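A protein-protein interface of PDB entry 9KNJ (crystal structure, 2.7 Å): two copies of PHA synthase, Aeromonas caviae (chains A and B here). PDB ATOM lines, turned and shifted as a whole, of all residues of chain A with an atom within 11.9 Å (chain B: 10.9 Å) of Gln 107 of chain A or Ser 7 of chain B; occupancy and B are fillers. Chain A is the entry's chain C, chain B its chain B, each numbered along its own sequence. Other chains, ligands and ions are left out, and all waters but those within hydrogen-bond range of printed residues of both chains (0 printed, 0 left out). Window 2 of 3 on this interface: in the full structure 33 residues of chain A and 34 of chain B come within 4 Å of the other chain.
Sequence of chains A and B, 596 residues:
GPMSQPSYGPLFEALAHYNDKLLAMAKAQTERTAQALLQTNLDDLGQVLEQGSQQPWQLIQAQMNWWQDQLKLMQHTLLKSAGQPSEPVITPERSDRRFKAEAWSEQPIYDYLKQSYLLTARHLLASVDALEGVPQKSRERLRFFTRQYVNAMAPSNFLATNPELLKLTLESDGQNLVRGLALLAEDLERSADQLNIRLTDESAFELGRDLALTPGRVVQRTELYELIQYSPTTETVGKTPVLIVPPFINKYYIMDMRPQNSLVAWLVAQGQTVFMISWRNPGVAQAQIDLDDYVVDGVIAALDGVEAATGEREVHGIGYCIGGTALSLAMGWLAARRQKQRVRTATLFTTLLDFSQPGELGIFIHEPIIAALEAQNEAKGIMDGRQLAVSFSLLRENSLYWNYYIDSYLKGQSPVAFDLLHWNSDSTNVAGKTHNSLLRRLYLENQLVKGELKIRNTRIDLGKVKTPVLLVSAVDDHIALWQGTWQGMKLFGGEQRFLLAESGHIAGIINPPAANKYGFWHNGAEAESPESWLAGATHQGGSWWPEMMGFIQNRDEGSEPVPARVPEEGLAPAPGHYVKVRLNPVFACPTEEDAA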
ATOM      1  N   LEU A  73       7.070  23.743  20.108  1.00  0.00           N
ATOM      2  CA  LEU A  73       6.985  23.083  18.810  1.00  0.00           C
ATOM      3  C   LEU A  73       5.923  21.998  18.815  1.00  0.00           C
ATOM      4  O   LEU A  73       5.215  21.800  17.824  1.00  0.00           O
ATOM      5  CB  LEU A  73       8.344  22.488  18.438  1.00  0.00           C
ATOM      6  CG  LEU A  73       8.411  21.677  17.142  1.00  0.00           C
ATOM      7  CD1 LEU A  73       8.791  22.569  15.978  1.00  0.00           C
ATOM      8  CD2 LEU A  73       9.395  20.520  17.274  1.00  0.00           C
ATOM      9  N   HIS A  76       2.597  23.425  18.659  1.00  0.00           N
ATOM     10  CA  HIS A  76       2.383  24.046  17.356  1.00  0.00           C
ATOM     11  C   HIS A  76       1.974  23.018  16.306  1.00  0.00           C
ATOM     12  O   HIS A  76       1.025  23.239  15.544  1.00  0.00           O
ATOM     13  CB  HIS A  76       3.652  24.790  16.933  1.00  0.00           C
ATOM     14  CG  HIS A  76       3.542  25.485  15.611  1.00  0.00           C
ATOM     15  ND1 HIS A  76       3.901  24.886  14.422  1.00  0.00           N
ATOM     16  CD2 HIS A  76       3.126  26.733  15.294  1.00  0.00           C
ATOM     17  CE1 HIS A  76       3.706  25.735  13.430  1.00  0.00           C
ATOM     18  NE2 HIS A  76       3.237  26.864  13.931  1.00  0.00           N
ATOM     19  N   THR A  77       2.676  21.882  16.252  1.00  0.00           N
ATOM     20  CA  THR A  77       2.362  20.871  15.245  1.00  0.00           C
ATOM     21  C   THR A  77       1.102  20.083  15.575  1.00  0.00           C
ATOM     22  O   THR A  77       0.432  19.598  14.658  1.00  0.00           O
ATOM     23  CB  THR A  77       3.537  19.907  15.058  1.00  0.00           C
ATOM     24  OG1 THR A  77       3.553  18.946  16.124  1.00  0.00           O
ATOM     25  CG2 THR A  77       4.861  20.660  14.989  1.00  0.00           C
ATOM     26  N   LYS A  80      -1.989  21.448  13.840  1.00  0.00           N
ATOM     27  CA  LYS A  80      -2.075  21.312  12.385  1.00  0.00           C
ATOM     28  C   LYS A  80      -2.467  22.626  11.715  1.00  0.00           C
ATOM     29  O   LYS A  80      -1.641  23.528  11.569  1.00  0.00           O
ATOM     30  CB  LYS A  80      -3.067  20.209  12.001  1.00  0.00           C
ATOM     31  CG  LYS A  80      -2.781  18.862  12.647  1.00  0.00           C
ATOM     32  CD  LYS A  80      -3.898  17.869  12.370  1.00  0.00           C
ATOM     33  CE  LYS A  80      -3.683  16.568  13.130  1.00  0.00           C
ATOM     34  NZ  LYS A  80      -4.745  15.568  12.824  1.00  0.00           N
ATOM     35  N   GLU A 106       8.531  18.007   3.888  1.00  0.00           N
ATOM     36  CA  GLU A 106       7.712  17.123   3.066  1.00  0.00           C
ATOM     37  C   GLU A 106       6.469  16.670   3.834  1.00  0.00           C
ATOM     38  O   GLU A 106       5.523  17.441   4.007  1.00  0.00           O
ATOM     39  CB  GLU A 106       8.530  15.915   2.603  1.00  0.00           C
ATOM     40  CG  GLU A 106       9.942  16.272   2.152  1.00  0.00           C
ATOM     41  CD  GLU A 106      10.801  15.050   1.892  1.00  0.00           C
ATOM     42  OE1 GLU A 106      10.231  13.966   1.639  1.00  0.00           O
ATOM     43  OE2 GLU A 106      12.045  15.173   1.945  1.00  0.00           O
ATOM     44  N   GLN A 107       6.478  15.420   4.288  1.00  0.00           N
ATOM     45  CA  GLN A 107       5.379  14.917   5.099  1.00  0.00           C
ATOM     46  C   GLN A 107       5.303  15.706   6.406  1.00  0.00           C
ATOM     47  O   GLN A 107       6.343  16.049   6.982  1.00  0.00           O
ATOM     48  CB  GLN A 107       5.569  13.422   5.381  1.00  0.00           C
ATOM     49  CG  GLN A 107       4.411  12.736   6.106  1.00  0.00           C
ATOM     50  CD  GLN A 107       3.350  12.190   5.165  1.00  0.00           C
ATOM     51  OE1 GLN A 107       3.359  12.471   3.967  1.00  0.00           O
ATOM     52  NE2 GLN A 107       2.428  11.399   5.708  1.00  0.00           N
ATOM     53  N   PRO A 108       4.100  16.020   6.898  1.00  0.00           N
ATOM     54  CA  PRO A 108       3.999  16.820   8.130  1.00  0.00           C
ATOM     55  C   PRO A 108       4.667  16.183   9.334  1.00  0.00           C
ATOM     56  O   PRO A 108       4.941  16.888  10.313  1.00  0.00           O
ATOM     57  CB  PRO A 108       2.484  16.955   8.339  1.00  0.00           C
ATOM     58  CG  PRO A 108       1.911  16.820   6.981  1.00  0.00           C
ATOM     59  CD  PRO A 108       2.786  15.835   6.257  1.00  0.00           C
ATOM     60  N   ILE A 109       4.933  14.877   9.306  1.00  0.00           N
ATOM     61  CA  ILE A 109       5.615  14.263  10.438  1.00  0.00           C
ATOM     62  C   ILE A 109       7.127  14.410  10.318  1.00  0.00           C
ATOM     63  O   ILE A 109       7.821  14.601  11.324  1.00  0.00           O
ATOM     64  CB  ILE A 109       5.194  12.794  10.593  1.00  0.00           C
ATOM     65  CG1 ILE A 109       5.898  12.199  11.802  1.00  0.00           C
ATOM     66  CG2 ILE A 109       5.522  11.994   9.349  1.00  0.00           C
ATOM     67  CD1 ILE A 109       5.130  11.119  12.443  1.00  0.00           C
ATOM     68  N   TYR A 110       7.666  14.319   9.102  1.00  0.00           N
ATOM     69  CA  TYR A 110       9.088  14.579   8.926  1.00  0.00           C
ATOM     70  C   TYR A 110       9.438  16.007   9.317  1.00  0.00           C
ATOM     71  O   TYR A 110      10.549  16.266   9.795  1.00  0.00           O
ATOM     72  CB  TYR A 110       9.506  14.301   7.480  1.00  0.00           C
ATOM     73  CG  TYR A 110      10.903  14.777   7.168  1.00  0.00           C
ATOM     74  CD1 TYR A 110      12.015  14.048   7.578  1.00  0.00           C
ATOM     75  CD2 TYR A 110      11.116  15.962   6.476  1.00  0.00           C
ATOM     76  CE1 TYR A 110      13.297  14.485   7.305  1.00  0.00           C
ATOM     77  CE2 TYR A 110      12.394  16.407   6.198  1.00  0.00           C
ATOM     78  CZ  TYR A 110      13.482  15.665   6.613  1.00  0.00           C
ATOM     79  OH  TYR A 110      14.753  16.112   6.333  1.00  0.00           O
ATOM     80  N   ASP A 111       8.506  16.945   9.125  1.00  0.00           N
ATOM     81  CA  ASP A 111       8.752  18.330   9.518  1.00  0.00           C
ATOM     82  C   ASP A 111       8.914  18.456  11.030  1.00  0.00           C
ATOM     83  O   ASP A 111       9.798  19.177  11.508  1.00  0.00           O
ATOM     84  CB  ASP A 111       7.619  19.230   9.020  1.00  0.00           C
ATOM     85  CG  ASP A 111       7.609  19.377   7.507  1.00  0.00           C
ATOM     86  OD1 ASP A 111       8.502  20.063   6.963  1.00  0.00           O
ATOM     87  OD2 ASP A 111       6.702  18.812   6.859  1.00  0.00           O
ATOM     88  N   TYR A 112       8.064  17.771  11.800  1.00  0.00           N
ATOM     89  CA  TYR A 112       8.229  17.777  13.250  1.00  0.00           C
ATOM     90  C   TYR A 112       9.507  17.056  13.656  1.00  0.00           C
ATOM     91  O   TYR A 112      10.203  17.487  14.582  1.00  0.00           O
ATOM     92  CB  TYR A 112       7.015  17.142  13.930  1.00  0.00           C
ATOM     93  CG  TYR A 112       7.180  16.974  15.423  1.00  0.00           C
ATOM     94  CD1 TYR A 112       6.960  18.037  16.290  1.00  0.00           C
ATOM     95  CD2 TYR A 112       7.556  15.753  15.968  1.00  0.00           C
ATOM     96  CE1 TYR A 112       7.111  17.889  17.660  1.00  0.00           C
ATOM     97  CE2 TYR A 112       7.712  15.596  17.334  1.00  0.00           C
ATOM     98  CZ  TYR A 112       7.488  16.666  18.173  1.00  0.00           C
ATOM     99  OH  TYR A 112       7.644  16.508  19.529  1.00  0.00           O
ATOM    100  N   LEU A 113       9.826  15.954  12.973  1.00  0.00           N
ATOM    101  CA  LEU A 113      11.049  15.216  13.270  1.00  0.00           C
ATOM    102  C   LEU A 113      12.286  16.071  13.029  1.00  0.00           C
ATOM    103  O   LEU A 113      13.207  16.091  13.855  1.00  0.00           O
ATOM    104  CB  LEU A 113      11.103  13.943  12.424  1.00  0.00           C
ATOM    105  CG  LEU A 113      11.820  12.733  13.022  1.00  0.00           C
ATOM    106  CD1 LEU A 113      11.451  12.564  14.479  1.00  0.00           C
ATOM    107  CD2 LEU A 113      11.487  11.474  12.238  1.00  0.00           C
ATOM    108  N   LYS A 114      12.322  16.788  11.904  1.00  0.00           N
ATOM    109  CA  LYS A 114      13.468  17.635  11.595  1.00  0.00           C
ATOM    110  C   LYS A 114      13.604  18.768  12.604  1.00  0.00           C
ATOM    111  O   LYS A 114      14.686  19.000  13.152  1.00  0.00           O
ATOM    112  CB  LYS A 114      13.336  18.190  10.176  1.00  0.00           C
ATOM    113  CG  LYS A 114      14.414  19.176   9.786  1.00  0.00           C
ATOM    114  CD  LYS A 114      14.297  19.566   8.320  1.00  0.00           C
ATOM    115  CE  LYS A 114      15.655  19.938   7.735  1.00  0.00           C
ATOM    116  NZ  LYS A 114      16.026  19.126   6.537  1.00  0.00           N
ATOM    117  N   GLN A 115      12.503  19.470  12.881  1.00  0.00           N
ATOM    118  CA  GLN A 115      12.578  20.643  13.746  1.00  0.00           C
ATOM    119  C   GLN A 115      13.023  20.271  15.155  1.00  0.00           C
ATOM    120  O   GLN A 115      13.820  20.990  15.769  1.00  0.00           O
ATOM    121  CB  GLN A 115      11.230  21.365  13.774  1.00  0.00           C
ATOM    122  CG  GLN A 115      10.873  22.069  12.469  1.00  0.00           C
ATOM    123  CD  GLN A 115      11.919  23.083  12.042  1.00  0.00           C
ATOM    124  OE1 GLN A 115      12.483  23.801  12.869  1.00  0.00           O
ATOM    125  NE2 GLN A 115      12.186  23.145  10.740  1.00  0.00           N
ATOM    126  N   SER A 116      12.519  19.152  15.688  1.00  0.00           N
ATOM    127  CA  SER A 116      12.963  18.705  17.005  1.00  0.00           C
ATOM    128  C   SER A 116      14.439  18.327  16.993  1.00  0.00           C
ATOM    129  O   SER A 116      15.123  18.456  18.015  1.00  0.00           O
ATOM    130  CB  SER A 116      12.114  17.525  17.482  1.00  0.00           C
ATOM    131  OG  SER A 116      11.725  16.705  16.398  1.00  0.00           O
ATOM    132  N   SER B   7       1.923   5.852   7.463  1.00  0.00           N
ATOM    133  CA  SER B   7       2.657   7.050   6.987  1.00  0.00           C
ATOM    134  C   SER B   7       4.097   7.009   7.501  1.00  0.00           C
ATOM    135  O   SER B   7       4.872   7.914   7.152  1.00  0.00           O
ATOM    136  CB  SER B   7       1.952   8.298   7.430  1.00  0.00           C
ATOM    137  OG  SER B   7       1.680   8.255   8.822  1.00  0.00           O
ATOM    138  N   TYR B   8       4.439   5.985   8.283  1.00  0.00           N
ATOM    139  CA  TYR B   8       5.791   5.904   8.891  1.00  0.00           C
ATOM    140  C   TYR B   8       6.662   4.932   8.095  1.00  0.00           C
ATOM    141  O   TYR B   8       7.898   5.021   8.187  1.00  0.00           O
ATOM    142  CB  TYR B   8       5.698   5.448  10.346  1.00  0.00           C
ATOM    143  CG  TYR B   8       4.944   6.365  11.278  1.00  0.00           C
ATOM    144  CD1 TYR B   8       4.235   7.458  10.808  1.00  0.00           C
ATOM    145  CD2 TYR B   8       4.964   6.153  12.644  1.00  0.00           C
ATOM    146  CE1 TYR B   8       3.542   8.295  11.664  1.00  0.00           C
ATOM    147  CE2 TYR B   8       4.285   6.987  13.516  1.00  0.00           C
ATOM    148  CZ  TYR B   8       3.571   8.062  13.026  1.00  0.00           C
ATOM    149  OH  TYR B   8       2.900   8.887  13.894  1.00  0.00           O
ATOM    150  N   GLY B   9       6.033   4.033   7.342  1.00  0.00           N
ATOM    151  CA  GLY B   9       6.783   3.034   6.558  1.00  0.00           C
ATOM    152  C   GLY B   9       7.906   3.639   5.735  1.00  0.00           C
ATOM    153  O   GLY B   9       9.074   3.351   6.047  1.00  0.00           O
ATOM    154  N   PRO B  10       7.640   4.479   4.710  1.00  0.00           N
ATOM    155  CA  PRO B  10       8.746   5.103   3.960  1.00  0.00           C
ATOM    156  C   PRO B  10       9.825   5.700   4.848  1.00  0.00           C
ATOM    157  O   PRO B  10      11.009   5.638   4.492  1.00  0.00           O
ATOM    158  CB  PRO B  10       8.054   6.185   3.115  1.00  0.00           C
ATOM    159  CG  PRO B  10       6.603   5.926   3.192  1.00  0.00           C
ATOM    160  CD  PRO B  10       6.312   4.949   4.276  1.00  0.00           C
ATOM    161  N   LEU B  11       9.454   6.279   5.993  1.00  0.00           N
ATOM    162  CA  LEU B  11      10.450   6.891   6.869  1.00  0.00           C
ATOM    163  C   LEU B  11      11.351   5.840   7.506  1.00  0.00           C
ATOM    164  O   LEU B  11      12.579   5.989   7.522  1.00  0.00           O
ATOM    165  CB  LEU B  11       9.762   7.739   7.941  1.00  0.00           C
ATOM    166  CG  LEU B  11       8.966   8.955   7.460  1.00  0.00           C
ATOM    167  CD1 LEU B  11       8.149   9.540   8.602  1.00  0.00           C
ATOM    168  CD2 LEU B  11       9.885  10.013   6.853  1.00  0.00           C
ATOM    169  N   PHE B  12      10.758   4.768   8.039  1.00  0.00           N
ATOM    170  CA  PHE B  12      11.555   3.697   8.628  1.00  0.00           C
ATOM    171  C   PHE B  12      12.419   3.005   7.581  1.00  0.00           C
ATOM    172  O   PHE B  12      13.577   2.661   7.850  1.00  0.00           O
ATOM    173  CB  PHE B  12      10.645   2.681   9.317  1.00  0.00           C
ATOM    174  CG  PHE B  12      10.301   3.041  10.727  1.00  0.00           C
ATOM    175  CD1 PHE B  12      11.234   2.886  11.739  1.00  0.00           C
ATOM    176  CD2 PHE B  12       9.045   3.529  11.045  1.00  0.00           C
ATOM    177  CE1 PHE B  12      10.924   3.216  13.041  1.00  0.00           C
ATOM    178  CE2 PHE B  12       8.725   3.858  12.349  1.00  0.00           C
ATOM    179  CZ  PHE B  12       9.667   3.703  13.348  1.00  0.00           C
ATOM    180  N   GLU B  13      11.866   2.778   6.387  1.00  0.00           N
ATOM    181  CA  GLU B  13      12.629   2.127   5.326  1.00  0.00           C
ATOM    182  C   GLU B  13      13.823   2.973   4.906  1.00  0.00           C
ATOM    183  O   GLU B  13      14.916   2.444   4.678  1.00  0.00           O
ATOM    184  CB  GLU B  13      11.726   1.840   4.127  1.00  0.00           C
ATOM    185  CG  GLU B  13      10.687   0.751   4.368  1.00  0.00           C
ATOM    186  CD  GLU B  13      10.065   0.240   3.082  1.00  0.00           C
ATOM    187  OE1 GLU B  13      10.636   0.498   2.000  1.00  0.00           O
ATOM    188  OE2 GLU B  13       9.005  -0.417   3.151  1.00  0.00           O
ATOM    189  N   ALA B  14      13.634   4.291   4.798  1.00  0.00           N
ATOM    190  CA  ALA B  14      14.746   5.172   4.454  1.00  0.00           C
ATOM    191  C   ALA B  14      15.807   5.178   5.548  1.00  0.00           C
ATOM    192  O   ALA B  14      17.006   5.250   5.255  1.00  0.00           O
ATOM    193  CB  ALA B  14      14.239   6.589   4.190  1.00  0.00           C
ATOM    194  N   LEU B  15      15.387   5.119   6.814  1.00  0.00           N
ATOM    195  CA  LEU B  15      16.352   5.074   7.908  1.00  0.00           C
ATOM    196  C   LEU B  15      17.195   3.808   7.838  1.00  0.00           C
ATOM    197  O   LEU B  15      18.428   3.865   7.909  1.00  0.00           O
ATOM    198  CB  LEU B  15      15.634   5.171   9.253  1.00  0.00           C
ATOM    199  CG  LEU B  15      15.361   6.598   9.732  1.00  0.00           C
ATOM    200  CD1 LEU B  15      14.376   6.604  10.892  1.00  0.00           C
ATOM    201  CD2 LEU B  15      16.664   7.290  10.110  1.00  0.00           C
ATOM    202  N   TRP B  67      17.433   9.582  15.177  1.00  0.00           N
ATOM    203  CA  TRP B  67      16.333   9.636  14.219  1.00  0.00           C
ATOM    204  C   TRP B  67      15.422   8.421  14.359  1.00  0.00           C
ATOM    205  O   TRP B  67      14.193   8.555  14.336  1.00  0.00           O
ATOM    206  CB  TRP B  67      16.870   9.735  12.789  1.00  0.00           C
ATOM    207  CG  TRP B  67      17.389  11.095  12.387  1.00  0.00           C
ATOM    208  CD1 TRP B  67      18.685  11.518  12.425  1.00  0.00           C
ATOM    209  CD2 TRP B  67      16.627  12.196  11.867  1.00  0.00           C
ATOM    210  NE1 TRP B  67      18.778  12.811  11.973  1.00  0.00           N
ATOM    211  CE2 TRP B  67      17.529  13.251  11.623  1.00  0.00           C
ATOM    212  CE3 TRP B  67      15.269  12.393  11.590  1.00  0.00           C
ATOM    213  CZ2 TRP B  67      17.120  14.484  11.114  1.00  0.00           C
ATOM    214  CZ3 TRP B  67      14.865  13.619  11.085  1.00  0.00           C
ATOM    215  CH2 TRP B  67      15.788  14.648  10.853  1.00  0.00           C
ATOM    216  N   LEU B  71      11.557   8.541  16.002  1.00  0.00           N
ATOM    217  CA  LEU B  71      10.429   8.141  15.163  1.00  0.00           C
ATOM    218  C   LEU B  71       9.676   6.964  15.772  1.00  0.00           C
ATOM    219  O   LEU B  71       8.444   6.901  15.692  1.00  0.00           O
ATOM    220  CB  LEU B  71      10.918   7.807  13.753  1.00  0.00           C
ATOM    221  CG  LEU B  71       9.863   7.437  12.710  1.00  0.00           C
ATOM    222  CD1 LEU B  71       9.110   8.671  12.244  1.00  0.00           C
ATOM    223  CD2 LEU B  71      10.523   6.744  11.531  1.00  0.00           C
ATOM    224  N   MET B  74       7.500   8.520  18.553  1.00  0.00           N
ATOM    225  CA  MET B  74       6.317   9.234  18.079  1.00  0.00           C
ATOM    226  C   MET B  74       5.225   8.278  17.619  1.00  0.00           C
ATOM    227  O   MET B  74       4.038   8.597  17.742  1.00  0.00           O
ATOM    228  CB  MET B  74       6.691  10.199  16.958  1.00  0.00           C
ATOM    229  CG  MET B  74       7.949  10.989  17.249  1.00  0.00           C
ATOM    230  SD  MET B  74       8.315  12.284  16.055  1.00  0.00           S
ATOM    231  CE  MET B  74       6.749  12.417  15.219  1.00  0.00           C
ATOM    232  N   GLN B  75       5.602   7.116  17.083  1.00  0.00           N
ATOM    233  CA  GLN B  75       4.613   6.090  16.769  1.00  0.00           C
ATOM    234  C   GLN B  75       3.882   5.631  18.025  1.00  0.00           C
ATOM    235  O   GLN B  75       2.649   5.526  18.040  1.00  0.00           O
ATOM    236  CB  GLN B  75       5.294   4.906  16.082  1.00  0.00           C
ATOM    237  CG  GLN B  75       4.346   3.976  15.348  1.00  0.00           C
ATOM    238  CD  GLN B  75       5.076   3.026  14.422  1.00  0.00           C
ATOM    239  OE1 GLN B  75       4.829   2.998  13.216  1.00  0.00           O
ATOM    240  NE2 GLN B  75       5.991   2.243  14.983  1.00  0.00           N
ATOM    241  N   LEU B  78       1.527   8.435  19.557  1.00  0.00           N
ATOM    242  CA  LEU B  78       0.319   8.656  18.765  1.00  0.00           C
ATOM    243  C   LEU B  78      -0.711   7.555  18.988  1.00  0.00           C
ATOM    244  O   LEU B  78      -1.914   7.787  18.819  1.00  0.00           O
ATOM    245  CB  LEU B  78       0.675   8.765  17.279  1.00  0.00           C
ATOM    246  CG  LEU B  78       1.050  10.140  16.709  1.00  0.00           C
ATOM    247  CD1 LEU B  78      -0.198  10.896  16.286  1.00  0.00           C
ATOM    248  CD2 LEU B  78       1.867  10.979  17.684  1.00  0.00           C
ATOM    249  N   LEU B  79      -0.265   6.361  19.368  1.00  0.00           N
ATOM    250  CA  LEU B  79      -1.166   5.258  19.687  1.00  0.00           C
ATOM    251  C   LEU B  79      -1.967   5.552  20.955  1.00  0.00           C
ATOM    252  O   LEU B  79      -1.422   5.578  22.060  1.00  0.00           O
ATOM    253  CB  LEU B  79      -0.375   3.957  19.848  1.00  0.00           C
ATOM    254  CG  LEU B  79      -0.454   2.941  18.703  1.00  0.00           C
ATOM    255  CD1 LEU B  79      -0.159   3.597  17.357  1.00  0.00           C
ATOM    256  CD2 LEU B  79       0.489   1.769  18.952  1.00  0.00           C
ATOM    257  N   ASN B 398      16.310  21.194   0.272  1.00  0.00           N
ATOM    258  CA  ASN B 398      15.312  20.548   1.164  1.00  0.00           C
ATOM    259  C   ASN B 398      15.993  19.757   2.280  1.00  0.00           C
ATOM    260  O   ASN B 398      15.530  19.861   3.427  1.00  0.00           O
ATOM    261  CB  ASN B 398      14.377  19.635   0.377  1.00  0.00           C
ATOM    262  CG  ASN B 398      13.537  20.392  -0.629  1.00  0.00           C
ATOM    263  OD1 ASN B 398      13.314  21.592  -0.482  1.00  0.00           O
ATOM    264  ND2 ASN B 398      13.061  19.699  -1.650  1.00  0.00           N
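Ser 7 of chain B touches Gln 107 of chain A (CB to NE2, 3.6 Å).
Ile 109 of chain A touches Tyr 8 of chain B (CD1 to CE1, 3.3 Å).
Ile 109 of chain A touches Leu 11 of chain B (CG2 to CD1, 3.7 Å).
Ile 109 of chain A touches Met 74 of chain B.
CD2 of Tyr 112 of chain A touches CE of Met 74 of chain B, 3.5 Å away.
Leu 113 of chain A touches Trp 67 of chain B.
CD2 of Leu 113 of chain A touches CD1 of Leu 71 of chain B, 3.7 Å away.
Leu 113 of chain A touches Met 74 of chain B (CD1 to SD, 3.5 Å).
Lys 114 of chain A touches Trp 67 of chain B.
Lys 80 of chain A touches none of the printed residues of chain B.
No residue of chain B comes within 4 Å of Glu 106 of chain A.
Of chain B, only Ser 7 (3.6 Å) comes within 4 Å of Gln 107 of chain A.
No residue of chain B comes within 4 Å of Pro 108 of chain A.
Ile 109 of chain A touches three residues of chain B.
No residue of chain B comes within 4 Å of Asp 111 of chain A.
Printed residues of chain B within 4 Å of Lys 114 of chain A: Trp 67 (3.9 Å) and Asn 398 (3.2 Å).
Printed residues of chain A within 4 Å of Ser 7 of chain B: Gln 107.
No residue of chain A comes within 4 Å of Gly 9 of chain B.
Of the printed residues of chain A, Leu 11 of chain B touches Ile 109.
Glu 13 of chain B touches none of the printed residues of chain A.
Of the printed residues of chain A, Met 74 of chain B touches Ile 109 (3.5 Å), Tyr 112 (3.5 Å) and Leu 113 (3.5 Å).
The nearest residue of chain B that does not touch Gln 107 of chain A is Leu 11 of chain B (5.5 Å).
No position is printed for both chains.
Of the 10 pairs that touch across the chains among the printed residues, none has its exchanged pair printed and touching as well.
Printed residues of chain A that touch a printed residue of chain B: Gln 107, Ile 109, Tyr 112, Leu 113 and Lys 114.
Hydrophobic or aromatic side chains of chain A within 4 Å of the printed part of chain B: Ile 109, Tyr 112 and Leu 113.
Of the 16 printed residues of chain B, 7 touch a printed residue of chain A.
Among the printed residues, 10 pairs touch across the chains.
Among the printed residues, no Asp or Glu carboxylate lies within 4 Å of a Lys or Arg side-chain nitrogen of the other chain.
The side-chain hydroxyl (OG) of Ser 116 of chain A lies within hydrogen-bond range of the backbone carbonyl oxygen (O) of Leu 113 of chain A, 3.0 Å away.
The backbone carbonyl oxygen of Tyr 112 of chain A is in hydrogen-bond range of the side-chain hydroxyl of Ser 116 of chain A (2.5 Å).
The side-chain amino group (NZ) of Lys 114 of chain A is in hydrogen-bond range of the side-chain hydroxyl (OH) of Tyr 110 of chain A, at 3.3 Å.
NZ of Lys 114 of chain A lies within hydrogen-bond range of O of Asn 398 of chain B (3.2 Å).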
